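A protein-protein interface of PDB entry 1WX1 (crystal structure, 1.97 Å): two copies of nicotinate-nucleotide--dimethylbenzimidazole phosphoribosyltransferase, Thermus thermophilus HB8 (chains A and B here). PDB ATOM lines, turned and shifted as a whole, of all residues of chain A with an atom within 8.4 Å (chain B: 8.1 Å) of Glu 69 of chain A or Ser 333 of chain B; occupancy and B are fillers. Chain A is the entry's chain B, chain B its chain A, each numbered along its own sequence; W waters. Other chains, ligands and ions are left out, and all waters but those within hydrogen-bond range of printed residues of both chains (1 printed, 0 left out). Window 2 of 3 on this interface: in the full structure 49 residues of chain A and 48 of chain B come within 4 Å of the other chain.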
ATOM      1  N   ASP A  55       1.416   6.113  10.957  1.00  0.00           N
ATOM      2  CA  ASP A  55       2.411   7.167  10.852  1.00  0.00           C
ATOM      3  C   ASP A  55       2.133   8.053   9.649  1.00  0.00           C
ATOM      4  O   ASP A  55       1.388   7.671   8.744  1.00  0.00           O
ATOM      5  CB  ASP A  55       3.820   6.574  10.785  1.00  0.00           C
ATOM      6  CG  ASP A  55       4.352   6.201  12.157  1.00  0.00           C
ATOM      7  OD1 ASP A  55       4.531   4.993  12.431  1.00  0.00           O
ATOM      8  OD2 ASP A  55       4.582   7.127  12.966  1.00  0.00           O
ATOM      9  N   VAL A  59       5.894  14.129   8.635  1.00  0.00           N
ATOM     10  CA  VAL A  59       6.852  14.365   9.708  1.00  0.00           C
ATOM     11  C   VAL A  59       8.145  14.904   9.098  1.00  0.00           C
ATOM     12  O   VAL A  59       8.949  15.540   9.777  1.00  0.00           O
ATOM     13  CB  VAL A  59       7.177  13.071  10.500  1.00  0.00           C
ATOM     14  CG1 VAL A  59       5.921  12.558  11.196  1.00  0.00           C
ATOM     15  CG2 VAL A  59       7.747  12.012   9.566  1.00  0.00           C
ATOM     16  N   ALA A  65       7.752  17.732  17.307  1.00  0.00           N
ATOM     17  CA  ALA A  65       8.958  17.729  18.124  1.00  0.00           C
ATOM     18  C   ALA A  65       9.379  16.301  18.453  1.00  0.00           C
ATOM     19  O   ALA A  65      10.509  16.060  18.875  1.00  0.00           O
ATOM     20  CB  ALA A  65       8.714  18.511  19.411  1.00  0.00           C
ATOM     21  N   TYR A  66       8.466  15.358  18.250  1.00  0.00           N
ATOM     22  CA  TYR A  66       8.733  13.955  18.544  1.00  0.00           C
ATOM     23  C   TYR A  66       9.129  13.142  17.319  1.00  0.00           C
ATOM     24  O   TYR A  66       8.631  13.378  16.219  1.00  0.00           O
ATOM     25  CB  TYR A  66       7.496  13.315  19.180  1.00  0.00           C
ATOM     26  CG  TYR A  66       7.115  13.912  20.513  1.00  0.00           C
ATOM     27  CD1 TYR A  66       7.848  13.619  21.662  1.00  0.00           C
ATOM     28  CD2 TYR A  66       6.024  14.773  20.626  1.00  0.00           C
ATOM     29  CE1 TYR A  66       7.502  14.165  22.895  1.00  0.00           C
ATOM     30  CE2 TYR A  66       5.671  15.327  21.853  1.00  0.00           C
ATOM     31  CZ  TYR A  66       6.413  15.017  22.982  1.00  0.00           C
ATOM     32  OH  TYR A  66       6.061  15.547  24.202  1.00  0.00           O
ATOM     33  N   PRO A  67      10.047  12.177  17.497  1.00  0.00           N
ATOM     34  CA  PRO A  67      10.510  11.315  16.404  1.00  0.00           C
ATOM     35  C   PRO A  67       9.353  10.420  15.967  1.00  0.00           C
ATOM     36  O   PRO A  67       8.479  10.096  16.774  1.00  0.00           O
ATOM     37  CB  PRO A  67      11.638  10.512  17.051  1.00  0.00           C
ATOM     38  CG  PRO A  67      12.144  11.426  18.118  1.00  0.00           C
ATOM     39  CD  PRO A  67      10.873  11.981  18.700  1.00  0.00           C
ATOM     40  N   GLN A  68       9.349  10.019  14.701  1.00  0.00           N
ATOM     41  CA  GLN A  68       8.283   9.173  14.173  1.00  0.00           C
ATOM     42  C   GLN A  68       8.143   7.856  14.935  1.00  0.00           C
ATOM     43  O   GLN A  68       7.042   7.314  15.057  1.00  0.00           O
ATOM     44  CB  GLN A  68       8.529   8.882  12.692  1.00  0.00           C
ATOM     45  CG  GLN A  68       7.397   8.121  12.018  1.00  0.00           C
ATOM     46  CD  GLN A  68       7.566   8.036  10.514  1.00  0.00           C
ATOM     47  OE1 GLN A  68       8.364   7.242  10.006  1.00  0.00           O
ATOM     48  NE2 GLN A  68       6.820   8.865   9.790  1.00  0.00           N
ATOM     49  N   GLU A  69       9.261   7.352  15.449  1.00  0.00           N
ATOM     50  CA  GLU A  69       9.281   6.094  16.193  1.00  0.00           C
ATOM     51  C   GLU A  69       8.339   6.073  17.400  1.00  0.00           C
ATOM     52  O   GLU A  69       7.933   5.005  17.855  1.00  0.00           O
ATOM     53  CB  GLU A  69      10.707   5.795  16.667  1.00  0.00           C
ATOM     54  CG  GLU A  69      11.352   6.952  17.410  1.00  0.00           C
ATOM     55  CD  GLU A  69      12.795   6.686  17.785  1.00  0.00           C
ATOM     56  OE1 GLU A  69      13.036   5.897  18.720  1.00  0.00           O
ATOM     57  OE2 GLU A  69      13.693   7.267  17.138  1.00  0.00           O
ATOM     58  N   VAL A  70       7.997   7.249  17.918  1.00  0.00           N
ATOM     59  CA  VAL A  70       7.116   7.335  19.080  1.00  0.00           C
ATOM     60  C   VAL A  70       5.754   6.682  18.848  1.00  0.00           C
ATOM     61  O   VAL A  70       5.169   6.123  19.771  1.00  0.00           O
ATOM     62  CB  VAL A  70       6.916   8.809  19.528  1.00  0.00           C
ATOM     63  CG1 VAL A  70       5.860   8.886  20.629  1.00  0.00           C
ATOM     64  CG2 VAL A  70       8.233   9.376  20.054  1.00  0.00           C
ATOM     65  N   THR A  71       5.246   6.743  17.621  1.00  0.00           N
ATOM     66  CA  THR A  71       3.951   6.136  17.320  1.00  0.00           C
ATOM     67  C   THR A  71       3.963   4.643  17.658  1.00  0.00           C
ATOM     68  O   THR A  71       3.108   4.154  18.399  1.00  0.00           O
ATOM     69  CB  THR A  71       3.577   6.301  15.830  1.00  0.00           C
ATOM     70  OG1 THR A  71       3.621   7.688  15.472  1.00  0.00           O
ATOM     71  CG2 THR A  71       2.171   5.774  15.568  1.00  0.00           C
ATOM     72  N   ARG A  72       4.940   3.921  17.120  1.00  0.00           N
ATOM     73  CA  ARG A  72       5.046   2.488  17.367  1.00  0.00           C
ATOM     74  C   ARG A  72       5.324   2.191  18.842  1.00  0.00           C
ATOM     75  O   ARG A  72       4.776   1.268  19.430  1.00  0.00           O
ATOM     76  CB  ARG A  72       6.181   1.938  16.502  1.00  0.00           C
ATOM     77  CG  ARG A  72       6.384   0.435  16.697  1.00  0.00           C
ATOM     78  CD  ARG A  72       7.520  -0.110  15.825  1.00  0.00           C
ATOM     79  NE  ARG A  72       7.718  -1.541  16.072  1.00  0.00           N
ATOM     80  CZ  ARG A  72       8.447  -1.887  17.150  1.00  0.00           C
ATOM     81  NH1 ARG A  72       8.947  -0.952  17.940  1.00  0.00           N
ATOM     82  NH2 ARG A  72       8.656  -3.178  17.419  1.00  0.00           N
ATOM     83  N   GLN A  73       6.194   2.988  19.455  1.00  0.00           N
ATOM     84  CA  GLN A  73       6.536   2.796  20.860  1.00  0.00           C
ATOM     85  C   GLN A  73       5.302   2.973  21.744  1.00  0.00           C
ATOM     86  O   GLN A  73       5.153   2.296  22.758  1.00  0.00           O
ATOM     87  CB  GLN A  73       7.617   3.790  21.283  1.00  0.00           C
ATOM     88  CG  GLN A  73       8.902   3.689  20.470  1.00  0.00           C
ATOM     89  CD  GLN A  73       9.904   4.765  20.834  1.00  0.00           C
ATOM     90  OE1 GLN A  73       9.531   5.903  21.127  1.00  0.00           O
ATOM     91  NE2 GLN A  73      11.189   4.418  20.795  1.00  0.00           N
ATOM     92  N   MET A  74       4.422   3.889  21.354  1.00  0.00           N
ATOM     93  CA  MET A  74       3.205   4.134  22.118  1.00  0.00           C
ATOM     94  C   MET A  74       2.198   3.002  21.944  1.00  0.00           C
ATOM     95  O   MET A  74       1.461   2.675  22.874  1.00  0.00           O
ATOM     96  CB  MET A  74       2.578   5.473  21.717  1.00  0.00           C
ATOM     97  CG  MET A  74       3.259   6.682  22.355  1.00  0.00           C
ATOM     98  SD  MET A  74       3.205   6.667  24.187  1.00  0.00           S
ATOM     99  CE  MET A  74       1.508   7.101  24.477  1.00  0.00           C
ATOM    100  N   VAL A  75       2.163   2.401  20.758  1.00  0.00           N
ATOM    101  CA  VAL A  75       1.246   1.293  20.520  1.00  0.00           C
ATOM    102  C   VAL A  75       1.612   0.163  21.476  1.00  0.00           C
ATOM    103  O   VAL A  75       0.738  -0.496  22.043  1.00  0.00           O
ATOM    104  CB  VAL A  75       1.333   0.780  19.062  1.00  0.00           C
ATOM    105  CG1 VAL A  75       0.559  -0.524  18.919  1.00  0.00           C
ATOM    106  CG2 VAL A  75       0.765   1.829  18.108  1.00  0.00           C
ATOM    107  N   LEU A  76       2.913  -0.056  21.651  1.00  0.00           N
ATOM    108  CA  LEU A  76       3.395  -1.097  22.554  1.00  0.00           C
ATOM    109  C   LEU A  76       3.019  -0.702  23.979  1.00  0.00           C
ATOM    110  O   LEU A  76       2.670  -1.549  24.801  1.00  0.00           O
ATOM    111  CB  LEU A  76       4.915  -1.243  22.432  1.00  0.00           C
ATOM    112  CG  LEU A  76       5.432  -1.679  21.056  1.00  0.00           C
ATOM    113  CD1 LEU A  76       6.958  -1.676  21.045  1.00  0.00           C
ATOM    114  CD2 LEU A  76       4.900  -3.060  20.730  1.00  0.00           C
ATOM    115  N   VAL A 103       1.316   1.971  10.879  1.00  0.00           N
ATOM    116  CA  VAL A 103       2.480   2.274  11.697  1.00  0.00           C
ATOM    117  C   VAL A 103       3.735   1.809  10.971  1.00  0.00           C
ATOM    118  O   VAL A 103       3.719   0.787  10.287  1.00  0.00           O
ATOM    119  CB  VAL A 103       2.415   1.554  13.063  1.00  0.00           C
ATOM    120  CG1 VAL A 103       3.723   1.759  13.823  1.00  0.00           C
ATOM    121  CG2 VAL A 103       1.237   2.084  13.877  1.00  0.00           C
ATOM    122  N   VAL A 104       4.816   2.568  11.112  1.00  0.00           N
ATOM    123  CA  VAL A 104       6.078   2.207  10.484  1.00  0.00           C
ATOM    124  C   VAL A 104       6.767   1.171  11.365  1.00  0.00           C
ATOM    125  O   VAL A 104       7.240   1.486  12.458  1.00  0.00           O
ATOM    126  CB  VAL A 104       7.010   3.429  10.333  1.00  0.00           C
ATOM    127  CG1 VAL A 104       8.395   2.974   9.885  1.00  0.00           C
ATOM    128  CG2 VAL A 104       6.433   4.407   9.317  1.00  0.00           C
ATOM    129  N   MET A 163      -3.533   7.768  17.386  1.00  0.00           N
ATOM    130  CA  MET A 163      -2.128   7.705  17.761  1.00  0.00           C
ATOM    131  C   MET A 163      -1.307   7.790  16.482  1.00  0.00           C
ATOM    132  O   MET A 163      -1.357   6.898  15.637  1.00  0.00           O
ATOM    133  CB  MET A 163      -1.798   6.409  18.509  1.00  0.00           C
ATOM    134  CG  MET A 163      -0.358   6.363  19.046  1.00  0.00           C
ATOM    135  SD  MET A 163       0.079   7.714  20.200  1.00  0.00           S
ATOM    136  CE  MET A 163       1.424   8.515  19.332  1.00  0.00           C
ATOM    137  N   ILE A 165       2.288  10.336  15.259  1.00  0.00           N
ATOM    138  CA  ILE A 165       3.091  11.544  15.292  1.00  0.00           C
ATOM    139  C   ILE A 165       2.845  12.334  14.010  1.00  0.00           C
ATOM    140  O   ILE A 165       2.996  11.804  12.906  1.00  0.00           O
ATOM    141  CB  ILE A 165       4.594  11.205  15.410  1.00  0.00           C
ATOM    142  CG1 ILE A 165       4.838  10.359  16.663  1.00  0.00           C
ATOM    143  CG2 ILE A 165       5.414  12.482  15.454  1.00  0.00           C
ATOM    144  CD1 ILE A 165       4.375  11.012  17.953  1.00  0.00           C
ATOM    145  N   THR B  17       4.439   9.187  29.953  1.00  0.00           N
ATOM    146  CA  THR B  17       4.382   9.090  28.499  1.00  0.00           C
ATOM    147  C   THR B  17       3.271   9.901  27.840  1.00  0.00           C
ATOM    148  O   THR B  17       2.242   9.366  27.426  1.00  0.00           O
ATOM    149  CB  THR B  17       4.275   7.615  28.042  1.00  0.00           C
ATOM    150  OG1 THR B  17       3.194   6.969  28.726  1.00  0.00           O
ATOM    151  CG2 THR B  17       5.578   6.875  28.342  1.00  0.00           C
ATOM    152  N   LYS B  18       3.507  11.203  27.741  1.00  0.00           N
ATOM    153  CA  LYS B  18       2.580  12.136  27.115  1.00  0.00           C
ATOM    154  C   LYS B  18       3.201  13.527  27.113  1.00  0.00           C
ATOM    155  O   LYS B  18       4.072  13.830  27.931  1.00  0.00           O
ATOM    156  CB  LYS B  18       1.226  12.138  27.843  1.00  0.00           C
ATOM    157  CG  LYS B  18       1.292  12.182  29.356  1.00  0.00           C
ATOM    158  CD  LYS B  18       1.565  13.572  29.876  1.00  0.00           C
ATOM    159  CE  LYS B  18       1.444  13.610  31.391  1.00  0.00           C
ATOM    160  NZ  LYS B  18       1.639  14.984  31.914  1.00  0.00           N
ATOM    161  N   PHE B 327       8.480   7.766  30.357  1.00  0.00           N
ATOM    162  CA  PHE B 327       9.212   7.555  29.108  1.00  0.00           C
ATOM    163  C   PHE B 327      10.249   6.452  29.292  1.00  0.00           C
ATOM    164  O   PHE B 327      10.357   5.532  28.476  1.00  0.00           O
ATOM    165  CB  PHE B 327       9.913   8.847  28.685  1.00  0.00           C
ATOM    166  CG  PHE B 327       8.977   9.898  28.158  1.00  0.00           C
ATOM    167  CD1 PHE B 327       8.392   9.758  26.904  1.00  0.00           C
ATOM    168  CD2 PHE B 327       8.686  11.030  28.910  1.00  0.00           C
ATOM    169  CE1 PHE B 327       7.518  10.727  26.407  1.00  0.00           C
ATOM    170  CE2 PHE B 327       7.814  12.005  28.423  1.00  0.00           C
ATOM    171  CZ  PHE B 327       7.233  11.856  27.168  1.00  0.00           C
ATOM    172  N   GLN B 328      10.996   6.551  30.386  1.00  0.00           N
ATOM    173  CA  GLN B 328      12.041   5.591  30.699  1.00  0.00           C
ATOM    174  C   GLN B 328      11.483   4.198  30.951  1.00  0.00           C
ATOM    175  O   GLN B 328      12.073   3.202  30.534  1.00  0.00           O
ATOM    176  CB  GLN B 328      12.823   6.076  31.921  1.00  0.00           C
ATOM    177  CG  GLN B 328      14.046   5.248  32.262  1.00  0.00           C
ATOM    178  CD  GLN B 328      14.904   5.907  33.327  1.00  0.00           C
ATOM    179  OE1 GLN B 328      14.455   6.131  34.454  1.00  0.00           O
ATOM    180  NE2 GLN B 328      16.144   6.226  32.974  1.00  0.00           N
ATOM    181  N   ALA B 330       8.553   2.939  29.798  1.00  0.00           N
ATOM    182  CA  ALA B 330       7.925   2.382  28.604  1.00  0.00           C
ATOM    183  C   ALA B 330       8.854   2.282  27.402  1.00  0.00           C
ATOM    184  O   ALA B 330       8.531   1.608  26.428  1.00  0.00           O
ATOM    185  CB  ALA B 330       6.696   3.209  28.232  1.00  0.00           C
ATOM    186  N   GLY B 331      10.001   2.950  27.464  1.00  0.00           N
ATOM    187  CA  GLY B 331      10.925   2.908  26.346  1.00  0.00           C
ATOM    188  C   GLY B 331      10.415   3.741  25.185  1.00  0.00           C
ATOM    189  O   GLY B 331      10.478   3.328  24.024  1.00  0.00           O
ATOM    190  N   VAL B 332       9.889   4.918  25.506  1.00  0.00           N
ATOM    191  CA  VAL B 332       9.371   5.834  24.499  1.00  0.00           C
ATOM    192  C   VAL B 332      10.374   6.975  24.365  1.00  0.00           C
ATOM    193  O   VAL B 332      10.846   7.503  25.371  1.00  0.00           O
ATOM    194  CB  VAL B 332       7.989   6.408  24.917  1.00  0.00           C
ATOM    195  CG1 VAL B 332       7.490   7.407  23.872  1.00  0.00           C
ATOM    196  CG2 VAL B 332       6.985   5.279  25.077  1.00  0.00           C
ATOM    197  N   SER B 333      10.708   7.336  23.126  1.00  0.00           N
ATOM    198  CA  SER B 333      11.667   8.411  22.842  1.00  0.00           C
ATOM    199  C   SER B 333      11.032   9.751  23.206  1.00  0.00           C
ATOM    200  O   SER B 333       9.820   9.880  23.184  1.00  0.00           O
ATOM    201  CB  SER B 333      12.041   8.416  21.367  1.00  0.00           C
ATOM    202  OG  SER B 333      12.520   7.144  20.964  1.00  0.00           O
ATOM    203  N   ARG B 334      11.839  10.775  23.474  1.00  0.00           N
ATOM    204  CA  ARG B 334      11.291  12.048  23.922  1.00  0.00           C
ATOM    205  C   ARG B 334      11.450  13.140  22.890  1.00  0.00           C
ATOM    206  O   ARG B 334      11.989  12.910  21.800  1.00  0.00           O
ATOM    207  CB  ARG B 334      11.960  12.475  25.192  1.00  0.00           C
ATOM    208  CG  ARG B 334      12.680  11.333  25.871  1.00  0.00           C
ATOM    209  CD  ARG B 334      13.476  11.846  27.040  1.00  0.00           C
ATOM    210  NE  ARG B 334      13.473  10.860  28.100  1.00  0.00           N
ATOM    211  CZ  ARG B 334      12.970  11.071  29.314  1.00  0.00           C
ATOM    212  NH1 ARG B 334      12.427  12.244  29.633  1.00  0.00           N
ATOM    213  NH2 ARG B 334      13.002  10.106  30.220  1.00  0.00           N
ATOM    214  N   GLY B 335      10.972  14.334  23.214  1.00  0.00           N
ATOM    215  CA  GLY B 335      11.141  15.461  22.330  1.00  0.00           C
ATOM    216  C   GLY B 335      11.301  16.817  22.989  1.00  0.00           C
ATOM    217  O   GLY B 335      12.383  17.443  22.818  1.00  0.00           O
ATOM    218  OXT GLY B 335      10.331  17.266  23.644  1.00  0.00           O
HETATM  219  O   HOH W   1       7.497   1.186  23.812  1.00  0.00           O
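The side-chain carboxylate (OE1) of Glu 69 of chain A is in hydrogen-bond range of the side-chain hydroxyl (OG) of Ser 333 of chain B, at 2.6 Å.
N of Ser 333 of chain B is in hydrogen-bond range of OE1 of Gln 73 of chain A (2.7 Å).
NE2 of Gln 73 of chain A sits at hydrogen-bond distance from O of Gly 331 of chain B.
Water W1 lies within hydrogen-bond range of O of Gln 73 of chain A (2.8 Å) and O of Ala 330 of chain B (2.8 Å).
Of chain B, only Ser 333 comes within 4 Å of Glu 69 of chain A.
Ser 333 of chain B touches three residues of chain A.
Of the printed residues of chain B, Ala 65 of chain A touches Gly 335.
Printed residues of chain B within 4 Å of Gln 73 of chain A: Gly 331 (3.5 Å), Val 332 (3.4 Å) and Ser 333 (2.7 Å).
Of the printed residues of chain B, Met 74 of chain A touches Thr 17 (3.8 Å).
Val 59 of chain A touches none of the printed residues of chain B.
The nearest residue of chain B that does not touch Glu 69 of chain A is Val 332 of chain B (6.3 Å).
The nearest residue of chain A that does not touch Ser 333 of chain B is Pro 67 of chain A (4.4 Å).
The nearest printed residue of chain A that does not touch Arg 334 of chain B is Ala 65 of chain A (4.5 Å).
Among the printed residues, pairs that only touch across the chains: Ala 65 of chain A with Gly 335 of chain B (3.6 Å), Tyr 66 of chain A with Arg 334 of chain B (3.8 Å), Tyr 66 of chain A with Gly 335 of chain B (3.5 Å), Pro 67 of chain A with Arg 334 of chain B (3.4 Å), Val 70 of chain A with Val 332 of chain B (3.9 Å), Val 70 of chain A with Ser 333 of chain B (3.5 Å), Gln 73 of chain A with Val 332 of chain B (3.4 Å) and Met 74 of chain A with Thr 17 of chain B (3.8 Å).
The backbone carbonyl oxygen (O) of Phe 327 of chain B is in hydrogen-bond range of the backbone NH (N) of Val 332 of chain B (3.1 Å).
OE1 of Glu 69 of chain A lies within hydrogen-bond range of NE2 of Gln 73 of chain A (3.1 Å).
Printed residues of chain B that touch a printed residue of chain A: Thr 17, Gly 331, Val 332, Ser 333, Arg 334 and Gly 335.
Of the 18 printed residues of chain A, 7 touch a printed residue of chain B.
Printed residues of chain A that touch a printed residue of chain B: Ala 65, Tyr 66, Pro 67, Glu 69, Val 70, Gln 73 and Met 74.
No position is printed for both chains.
Of the 11 pairs that touch across the chains among the printed residues, none has its exchanged pair printed and touching as well.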
